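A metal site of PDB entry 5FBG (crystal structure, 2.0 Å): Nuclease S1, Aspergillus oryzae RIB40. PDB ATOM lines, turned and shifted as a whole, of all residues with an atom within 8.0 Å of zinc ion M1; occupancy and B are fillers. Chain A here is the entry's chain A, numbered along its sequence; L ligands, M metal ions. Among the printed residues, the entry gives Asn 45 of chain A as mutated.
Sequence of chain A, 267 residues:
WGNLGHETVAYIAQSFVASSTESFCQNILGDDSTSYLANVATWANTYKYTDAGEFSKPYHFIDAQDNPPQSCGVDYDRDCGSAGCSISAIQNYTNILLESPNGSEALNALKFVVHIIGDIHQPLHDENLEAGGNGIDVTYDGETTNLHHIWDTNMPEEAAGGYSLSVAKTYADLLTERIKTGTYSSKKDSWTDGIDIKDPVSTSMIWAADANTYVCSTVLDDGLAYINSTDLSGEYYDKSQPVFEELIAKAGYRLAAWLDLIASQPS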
ATOM      1  N   TRP A   1     -22.555   7.742 -20.372  1.00  0.00           N
ATOM      2  CA  TRP A   1     -23.078   6.766 -21.273  1.00  0.00           C
ATOM      3  C   TRP A   1     -23.896   7.456 -22.359  1.00  0.00           C
ATOM      4  O   TRP A   1     -24.434   8.548 -22.144  1.00  0.00           O
ATOM      5  CB  TRP A   1     -23.946   5.711 -20.594  1.00  0.00           C
ATOM      6  CG  TRP A   1     -23.291   5.070 -19.400  1.00  0.00           C
ATOM      7  CD1 TRP A   1     -23.534   5.348 -18.118  1.00  0.00           C
ATOM      8  CD2 TRP A   1     -22.268   4.035 -19.414  1.00  0.00           C
ATOM      9  NE1 TRP A   1     -22.788   4.511 -17.306  1.00  0.00           N
ATOM     10  CE2 TRP A   1     -22.003   3.700 -18.098  1.00  0.00           C
ATOM     11  CE3 TRP A   1     -21.592   3.356 -20.442  1.00  0.00           C
ATOM     12  CZ2 TRP A   1     -21.015   2.744 -17.741  1.00  0.00           C
ATOM     13  CZ3 TRP A   1     -20.644   2.389 -20.097  1.00  0.00           C
ATOM     14  CH2 TRP A   1     -20.356   2.091 -18.756  1.00  0.00           C
ATOM     15  N   GLY A   2     -24.072   6.723 -23.457  1.00  0.00           N
ATOM     16  CA  GLY A   2     -25.078   7.057 -24.453  1.00  0.00           C
ATOM     17  C   GLY A   2     -26.469   6.616 -23.958  1.00  0.00           C
ATOM     18  O   GLY A   2     -26.653   6.196 -22.807  1.00  0.00           O
ATOM     19  N   HIS A   6     -27.750   4.647 -20.333  1.00  0.00           N
ATOM     20  CA  HIS A   6     -28.586   5.329 -19.364  1.00  0.00           C
ATOM     21  C   HIS A   6     -29.938   4.639 -19.154  1.00  0.00           C
ATOM     22  O   HIS A   6     -30.404   4.556 -18.026  1.00  0.00           O
ATOM     23  CB  HIS A   6     -28.818   6.813 -19.695  1.00  0.00           C
ATOM     24  CG  HIS A   6     -27.613   7.649 -19.439  1.00  0.00           C
ATOM     25  ND1 HIS A   6     -27.213   7.980 -18.183  1.00  0.00           N
ATOM     26  CD2 HIS A   6     -26.669   8.143 -20.289  1.00  0.00           C
ATOM     27  CE1 HIS A   6     -26.053   8.619 -18.238  1.00  0.00           C
ATOM     28  NE2 HIS A   6     -25.698   8.721 -19.500  1.00  0.00           N
ATOM     29  N   ASN A  45     -28.773  15.133 -20.506  1.00  0.00           N
ATOM     30  CA  ASN A  45     -28.064  15.398 -21.719  1.00  0.00           C
ATOM     31  C   ASN A  45     -28.806  16.373 -22.611  1.00  0.00           C
ATOM     32  O   ASN A  45     -28.241  17.349 -23.074  1.00  0.00           O
ATOM     33  CB  ASN A  45     -27.695  14.128 -22.491  1.00  0.00           C
ATOM     34  CG  ASN A  45     -26.498  13.414 -21.898  1.00  0.00           C
ATOM     35  OD1 ASN A  45     -25.821  13.947 -21.041  1.00  0.00           O
ATOM     36  ND2 ASN A  45     -26.288  12.207 -22.320  1.00  0.00           N
ATOM     37  N   LYS A  48     -28.623  19.986 -21.067  1.00  0.00           N
ATOM     38  CA  LYS A  48     -27.316  20.687 -21.074  1.00  0.00           C
ATOM     39  C   LYS A  48     -27.050  21.452 -22.419  1.00  0.00           C
ATOM     40  O   LYS A  48     -26.228  22.384 -22.435  1.00  0.00           O
ATOM     41  CB  LYS A  48     -26.160  19.761 -20.737  1.00  0.00           C
ATOM     42  CG  LYS A  48     -25.725  18.867 -21.890  1.00  0.00           C
ATOM     43  CD  LYS A  48     -24.781  17.801 -21.345  1.00  0.00           C
ATOM     44  CE  LYS A  48     -24.173  16.844 -22.336  1.00  0.00           C
ATOM     45  NZ  LYS A  48     -23.395  15.741 -21.643  1.00  0.00           N
ATOM     46  N   HIS A  60     -21.855  16.350 -15.418  1.00  0.00           N
ATOM     47  CA  HIS A  60     -21.855  14.993 -15.929  1.00  0.00           C
ATOM     48  C   HIS A  60     -20.609  14.186 -15.647  1.00  0.00           C
ATOM     49  O   HIS A  60     -20.560  12.941 -15.954  1.00  0.00           O
ATOM     50  CB  HIS A  60     -22.106  15.047 -17.462  1.00  0.00           C
ATOM     51  CG  HIS A  60     -23.474  15.542 -17.782  1.00  0.00           C
ATOM     52  ND1 HIS A  60     -24.435  14.740 -18.369  1.00  0.00           N
ATOM     53  CD2 HIS A  60     -24.092  16.707 -17.443  1.00  0.00           C
ATOM     54  CE1 HIS A  60     -25.561  15.419 -18.456  1.00  0.00           C
ATOM     55  NE2 HIS A  60     -25.399  16.598 -17.862  1.00  0.00           N
ATOM     56  N   PHE A  61     -19.592  14.842 -15.079  1.00  0.00           N
ATOM     57  CA  PHE A  61     -18.281  14.191 -14.887  1.00  0.00           C
ATOM     58  C   PHE A  61     -17.527  14.826 -13.746  1.00  0.00           C
ATOM     59  O   PHE A  61     -17.905  15.858 -13.163  1.00  0.00           O
ATOM     60  CB  PHE A  61     -17.481  14.195 -16.221  1.00  0.00           C
ATOM     61  CG  PHE A  61     -17.327  15.566 -16.801  1.00  0.00           C
ATOM     62  CD1 PHE A  61     -16.319  16.421 -16.347  1.00  0.00           C
ATOM     63  CD2 PHE A  61     -18.203  16.007 -17.800  1.00  0.00           C
ATOM     64  CE1 PHE A  61     -16.194  17.686 -16.859  1.00  0.00           C
ATOM     65  CE2 PHE A  61     -18.087  17.279 -18.338  1.00  0.00           C
ATOM     66  CZ  PHE A  61     -17.097  18.129 -17.871  1.00  0.00           C
ATOM     67  N   HIS A 115     -29.749  10.290 -14.205  1.00  0.00           N
ATOM     68  CA  HIS A 115     -28.753  10.355 -15.253  1.00  0.00           C
ATOM     69  C   HIS A 115     -27.309  10.304 -14.676  1.00  0.00           C
ATOM     70  O   HIS A 115     -26.472   9.566 -15.158  1.00  0.00           O
ATOM     71  CB  HIS A 115     -28.924  11.635 -16.090  1.00  0.00           C
ATOM     72  CG  HIS A 115     -27.943  11.742 -17.214  1.00  0.00           C
ATOM     73  ND1 HIS A 115     -28.162  11.175 -18.432  1.00  0.00           N
ATOM     74  CD2 HIS A 115     -26.720  12.329 -17.290  1.00  0.00           C
ATOM     75  CE1 HIS A 115     -27.135  11.411 -19.231  1.00  0.00           C
ATOM     76  NE2 HIS A 115     -26.254  12.120 -18.562  1.00  0.00           N
ATOM     77  N   ASP A 119     -23.831   8.218 -15.156  1.00  0.00           N
ATOM     78  CA  ASP A 119     -22.584   8.791 -15.752  1.00  0.00           C
ATOM     79  C   ASP A 119     -21.338   8.571 -14.864  1.00  0.00           C
ATOM     80  O   ASP A 119     -20.274   8.237 -15.376  1.00  0.00           O
ATOM     81  CB  ASP A 119     -22.746  10.279 -15.999  1.00  0.00           C
ATOM     82  CG  ASP A 119     -23.151  10.644 -17.390  1.00  0.00           C
ATOM     83  OD1 ASP A 119     -23.228   9.760 -18.299  1.00  0.00           O
ATOM     84  OD2 ASP A 119     -23.445  11.851 -17.539  1.00  0.00           O
ATOM     85  N   GLN A 122     -19.396   5.407 -15.617  1.00  0.00           N
ATOM     86  CA  GLN A 122     -18.670   5.306 -16.860  1.00  0.00           C
ATOM     87  C   GLN A 122     -17.251   5.825 -16.529  1.00  0.00           C
ATOM     88  O   GLN A 122     -17.119   6.998 -16.211  1.00  0.00           O
ATOM     89  CB  GLN A 122     -19.331   6.167 -17.949  1.00  0.00           C
ATOM     90  CG  GLN A 122     -19.081   5.722 -19.376  1.00  0.00           C
ATOM     91  CD  GLN A 122     -17.651   6.075 -19.916  1.00  0.00           C
ATOM     92  OE1 GLN A 122     -16.650   5.579 -19.376  1.00  0.00           O
ATOM     93  NE2 GLN A 122     -17.586   6.868 -20.945  1.00  0.00           N
ATOM     94  N   LEU A 124     -14.507   6.853 -17.855  1.00  0.00           N
ATOM     95  CA  LEU A 124     -14.014   8.098 -18.477  1.00  0.00           C
ATOM     96  C   LEU A 124     -14.738   9.390 -18.069  1.00  0.00           C
ATOM     97  O   LEU A 124     -14.255  10.509 -18.327  1.00  0.00           O
ATOM     98  CB  LEU A 124     -13.914   7.963 -19.973  1.00  0.00           C
ATOM     99  CG  LEU A 124     -12.697   7.129 -20.443  1.00  0.00           C
ATOM    100  CD1 LEU A 124     -12.783   6.805 -21.922  1.00  0.00           C
ATOM    101  CD2 LEU A 124     -11.376   7.866 -20.136  1.00  0.00           C
ATOM    102  N   HIS A 125     -15.870   9.245 -17.364  1.00  0.00           N
ATOM    103  CA  HIS A 125     -16.515  10.395 -16.658  1.00  0.00           C
ATOM    104  C   HIS A 125     -15.885  10.694 -15.328  1.00  0.00           C
ATOM    105  O   HIS A 125     -16.360  11.559 -14.593  1.00  0.00           O
ATOM    106  CB  HIS A 125     -18.012  10.050 -16.455  1.00  0.00           C
ATOM    107  CG  HIS A 125     -18.839  10.280 -17.687  1.00  0.00           C
ATOM    108  ND1 HIS A 125     -19.752  11.307 -17.759  1.00  0.00           N
ATOM    109  CD2 HIS A 125     -18.849   9.672 -18.880  1.00  0.00           C
ATOM    110  CE1 HIS A 125     -20.280  11.326 -18.965  1.00  0.00           C
ATOM    111  NE2 HIS A 125     -19.769  10.336 -19.652  1.00  0.00           N
ATOM    112  N   ALA A 131     -10.091  15.561 -21.958  1.00  0.00           N
ATOM    113  CA  ALA A 131     -11.504  15.772 -21.703  1.00  0.00           C
ATOM    114  C   ALA A 131     -12.288  14.471 -21.556  1.00  0.00           C
ATOM    115  O   ALA A 131     -13.195  14.212 -22.346  1.00  0.00           O
ATOM    116  CB  ALA A 131     -12.086  16.657 -22.814  1.00  0.00           C
ATOM    117  N   GLY A 132     -11.860  13.638 -20.602  1.00  0.00           N
ATOM    118  CA  GLY A 132     -12.456  12.329 -20.407  1.00  0.00           C
ATOM    119  C   GLY A 132     -12.321  11.377 -21.593  1.00  0.00           C
ATOM    120  O   GLY A 132     -13.192  10.566 -21.867  1.00  0.00           O
ATOM    121  N   ASN A 134     -12.317  12.277 -24.684  1.00  0.00           N
ATOM    122  CA  ASN A 134     -12.927  12.808 -25.915  1.00  0.00           C
ATOM    123  C   ASN A 134     -11.892  13.175 -26.984  1.00  0.00           C
ATOM    124  O   ASN A 134     -12.147  13.029 -28.150  1.00  0.00           O
ATOM    125  CB  ASN A 134     -13.850  13.988 -25.613  1.00  0.00           C
ATOM    126  CG  ASN A 134     -15.256  13.515 -25.159  1.00  0.00           C
ATOM    127  OD1 ASN A 134     -16.043  13.002 -25.972  1.00  0.00           O
ATOM    128  ND2 ASN A 134     -15.530  13.618 -23.857  1.00  0.00           N
ATOM    129  N   HIS A 148     -13.786   8.104 -25.577  1.00  0.00           N
ATOM    130  CA  HIS A 148     -14.908   8.362 -24.710  1.00  0.00           C
ATOM    131  C   HIS A 148     -16.195   7.779 -25.359  1.00  0.00           C
ATOM    132  O   HIS A 148     -16.998   7.082 -24.703  1.00  0.00           O
ATOM    133  CB  HIS A 148     -15.105   9.837 -24.485  1.00  0.00           C
ATOM    134  CG  HIS A 148     -16.176  10.146 -23.492  1.00  0.00           C
ATOM    135  ND1 HIS A 148     -15.891  10.495 -22.184  1.00  0.00           N
ATOM    136  CD2 HIS A 148     -17.531  10.107 -23.584  1.00  0.00           C
ATOM    137  CE1 HIS A 148     -17.039  10.673 -21.521  1.00  0.00           C
ATOM    138  NE2 HIS A 148     -18.028  10.486 -22.365  1.00  0.00           N
ATOM    139  N   HIS A 149     -16.341   8.034 -26.652  1.00  0.00           N
ATOM    140  CA  HIS A 149     -17.532   7.609 -27.386  1.00  0.00           C
ATOM    141  C   HIS A 149     -17.732   6.116 -27.447  1.00  0.00           C
ATOM    142  O   HIS A 149     -18.877   5.619 -27.336  1.00  0.00           O
ATOM    143  CB  HIS A 149     -17.546   8.191 -28.797  1.00  0.00           C
ATOM    144  CG  HIS A 149     -18.876   8.085 -29.485  1.00  0.00           C
ATOM    145  ND1 HIS A 149     -19.232   7.020 -30.282  1.00  0.00           N
ATOM    146  CD2 HIS A 149     -19.941   8.926 -29.498  1.00  0.00           C
ATOM    147  CE1 HIS A 149     -20.442   7.213 -30.773  1.00  0.00           C
ATOM    148  NE2 HIS A 149     -20.894   8.353 -30.299  1.00  0.00           N
ATOM    149  N   TRP A 151     -16.702   3.959 -25.155  1.00  0.00           N
ATOM    150  CA  TRP A 151     -17.160   3.563 -23.809  1.00  0.00           C
ATOM    151  C   TRP A 151     -18.649   3.937 -23.563  1.00  0.00           C
ATOM    152  O   TRP A 151     -19.395   3.162 -22.986  1.00  0.00           O
ATOM    153  CB  TRP A 151     -16.223   4.101 -22.711  1.00  0.00           C
ATOM    154  CG  TRP A 151     -15.038   3.185 -22.544  1.00  0.00           C
ATOM    155  CD1 TRP A 151     -13.866   3.220 -23.252  1.00  0.00           C
ATOM    156  CD2 TRP A 151     -14.945   2.084 -21.665  1.00  0.00           C
ATOM    157  NE1 TRP A 151     -13.075   2.203 -22.889  1.00  0.00           N
ATOM    158  CE2 TRP A 151     -13.689   1.477 -21.898  1.00  0.00           C
ATOM    159  CE3 TRP A 151     -15.790   1.560 -20.680  1.00  0.00           C
ATOM    160  CZ2 TRP A 151     -13.271   0.343 -21.202  1.00  0.00           C
ATOM    161  CZ3 TRP A 151     -15.351   0.430 -19.960  1.00  0.00           C
ATOM    162  CH2 TRP A 151     -14.113  -0.163 -20.244  1.00  0.00           C
ATOM    163  N   ASP A 152     -19.055   5.098 -24.056  1.00  0.00           N
ATOM    164  CA  ASP A 152     -20.417   5.577 -23.849  1.00  0.00           C
ATOM    165  C   ASP A 152     -21.433   4.732 -24.668  1.00  0.00           C
ATOM    166  O   ASP A 152     -22.489   4.369 -24.161  1.00  0.00           O
ATOM    167  CB  ASP A 152     -20.570   7.044 -24.274  1.00  0.00           C
ATOM    168  CG  ASP A 152     -20.453   8.053 -23.138  1.00  0.00           C
ATOM    169  OD1 ASP A 152     -20.126   7.751 -21.989  1.00  0.00           O
ATOM    170  OD2 ASP A 152     -20.631   9.246 -23.455  1.00  0.00           O
ATOM    171  N   THR A 153     -21.060   4.399 -25.901  1.00  0.00           N
ATOM    172  CA  THR A 153     -22.019   4.065 -26.954  1.00  0.00           C
ATOM    173  C   THR A 153     -21.652   2.833 -27.785  1.00  0.00           C
ATOM    174  O   THR A 153     -22.355   1.820 -27.746  1.00  0.00           O
ATOM    175  CB  THR A 153     -22.255   5.318 -27.822  1.00  0.00           C
ATOM    176  OG1 THR A 153     -22.823   6.312 -26.951  1.00  0.00           O
ATOM    177  CG2 THR A 153     -23.188   5.076 -29.007  1.00  0.00           C
HETATM  178  P1  LIG L   1     -22.894  12.009 -21.475  1.00  0.00           P
HETATM  179  O1  LIG L   1     -23.911  11.048 -20.913  1.00  0.00           O
HETATM  180  O2  LIG L   1     -22.742  13.167 -20.483  1.00  0.00           O
HETATM  181  O3  LIG L   1     -21.579  11.360 -21.762  1.00  0.00           O
HETATM  182  O4  LIG L   1     -23.238  12.707 -22.771  1.00  0.00           O
HETATM  183  N1  LG2 L   2     -17.311  14.477 -20.994  1.00  0.00           N
HETATM  184  C1  LG2 L   2     -16.634  13.919 -19.902  1.00  0.00           C
HETATM  185  N2  LG2 L   2     -15.525  14.562 -19.407  1.00  0.00           N
HETATM  186  C2  LG2 L   2     -15.131  15.729 -19.931  1.00  0.00           C
HETATM  187  C3  LG2 L   2     -15.810  16.318 -21.060  1.00  0.00           C
HETATM  188  C4  LG2 L   2     -16.869  15.662 -21.568  1.00  0.00           C
HETATM  189  O1  LG2 L   2     -17.100  12.912 -19.375  1.00  0.00           O
HETATM  190  N3  LG2 L   2     -14.105  16.349 -19.382  1.00  0.00           N
HETATM  191  C5  LG2 L   2     -18.556  13.835 -21.465  1.00  0.00           C
HETATM  192  C6  LG2 L   2     -19.789  14.746 -21.447  1.00  0.00           C
HETATM  193  C7  LG2 L   2     -19.980  15.145 -22.927  1.00  0.00           C
HETATM  194  C8  LG2 L   2     -19.423  13.927 -23.643  1.00  0.00           C
HETATM  195  O2  LG2 L   2     -18.348  13.445 -22.802  1.00  0.00           O
HETATM  196  O3  LG2 L   2     -21.321  15.292 -23.408  1.00  0.00           O
HETATM  197  C9  LG2 L   2     -18.905  14.161 -25.059  1.00  0.00           C
HETATM  198  O4  LG2 L   2     -18.743  12.866 -25.664  1.00  0.00           O
HETATM  199 ZN    ZN M   1     -20.046  10.286 -21.773  1.00  0.00          ZN
HETATM  200 ZN    ZN M   2     -23.935   9.379 -20.201  1.00  0.00          ZN
HETATM  201 ZN    ZN M   3     -24.364  12.854 -19.195  1.00  0.00          ZN
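An oxygen (O2) of LG2 L2 lies close to a ring nitrogen (NE2) of His 148 (3.0 Å).
A ring nitrogen (ND1) of His 125 sits at hydrogen-bond distance from an oxygen (O1) of LG2 L2, at 3.5 Å.
An oxygen (O3) of LG2 L2 lies within hydrogen-bond range of the side-chain amino group (NZ) of Lys 48 (2.8 Å).
The side-chain amide oxygen (OD1) of Asn 134 is in hydrogen-bond range of an oxygen (O4) of LG2 L2, 2.7 Å away.
NE2 of Gln 122 lies close to OD1 of Asp 152 (2.9 Å).
A ring nitrogen (ND1) of His 148 is in hydrogen-bond range of the backbone carbonyl oxygen (O) of Gly 132 (2.7 Å).
O of His 60 lies within hydrogen-bond range of ND1 of His 125.
The backbone carbonyl oxygen (O) of Asp 152 sits at hydrogen-bond distance from the backbone NH (N) of Gly 2, 2.9 Å away.
Merely in contact with zinc ion M1: Trp 1.
Within 4 Å of zinc ion M1: Trp 1, His 125, His 148 and Asp 152.
O3 of LIG L1 is bound to zinc ion M1, at 1.9 Å.
OD2 of Asp 152 binds zinc ion M1.
NE2 of His 148 binds zinc ion M1, at 2.1 Å.
NE2 of His 125 is bound to zinc ion M1 (2.1 Å).
OD1 of Asp 152 is bound to zinc ion M1.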
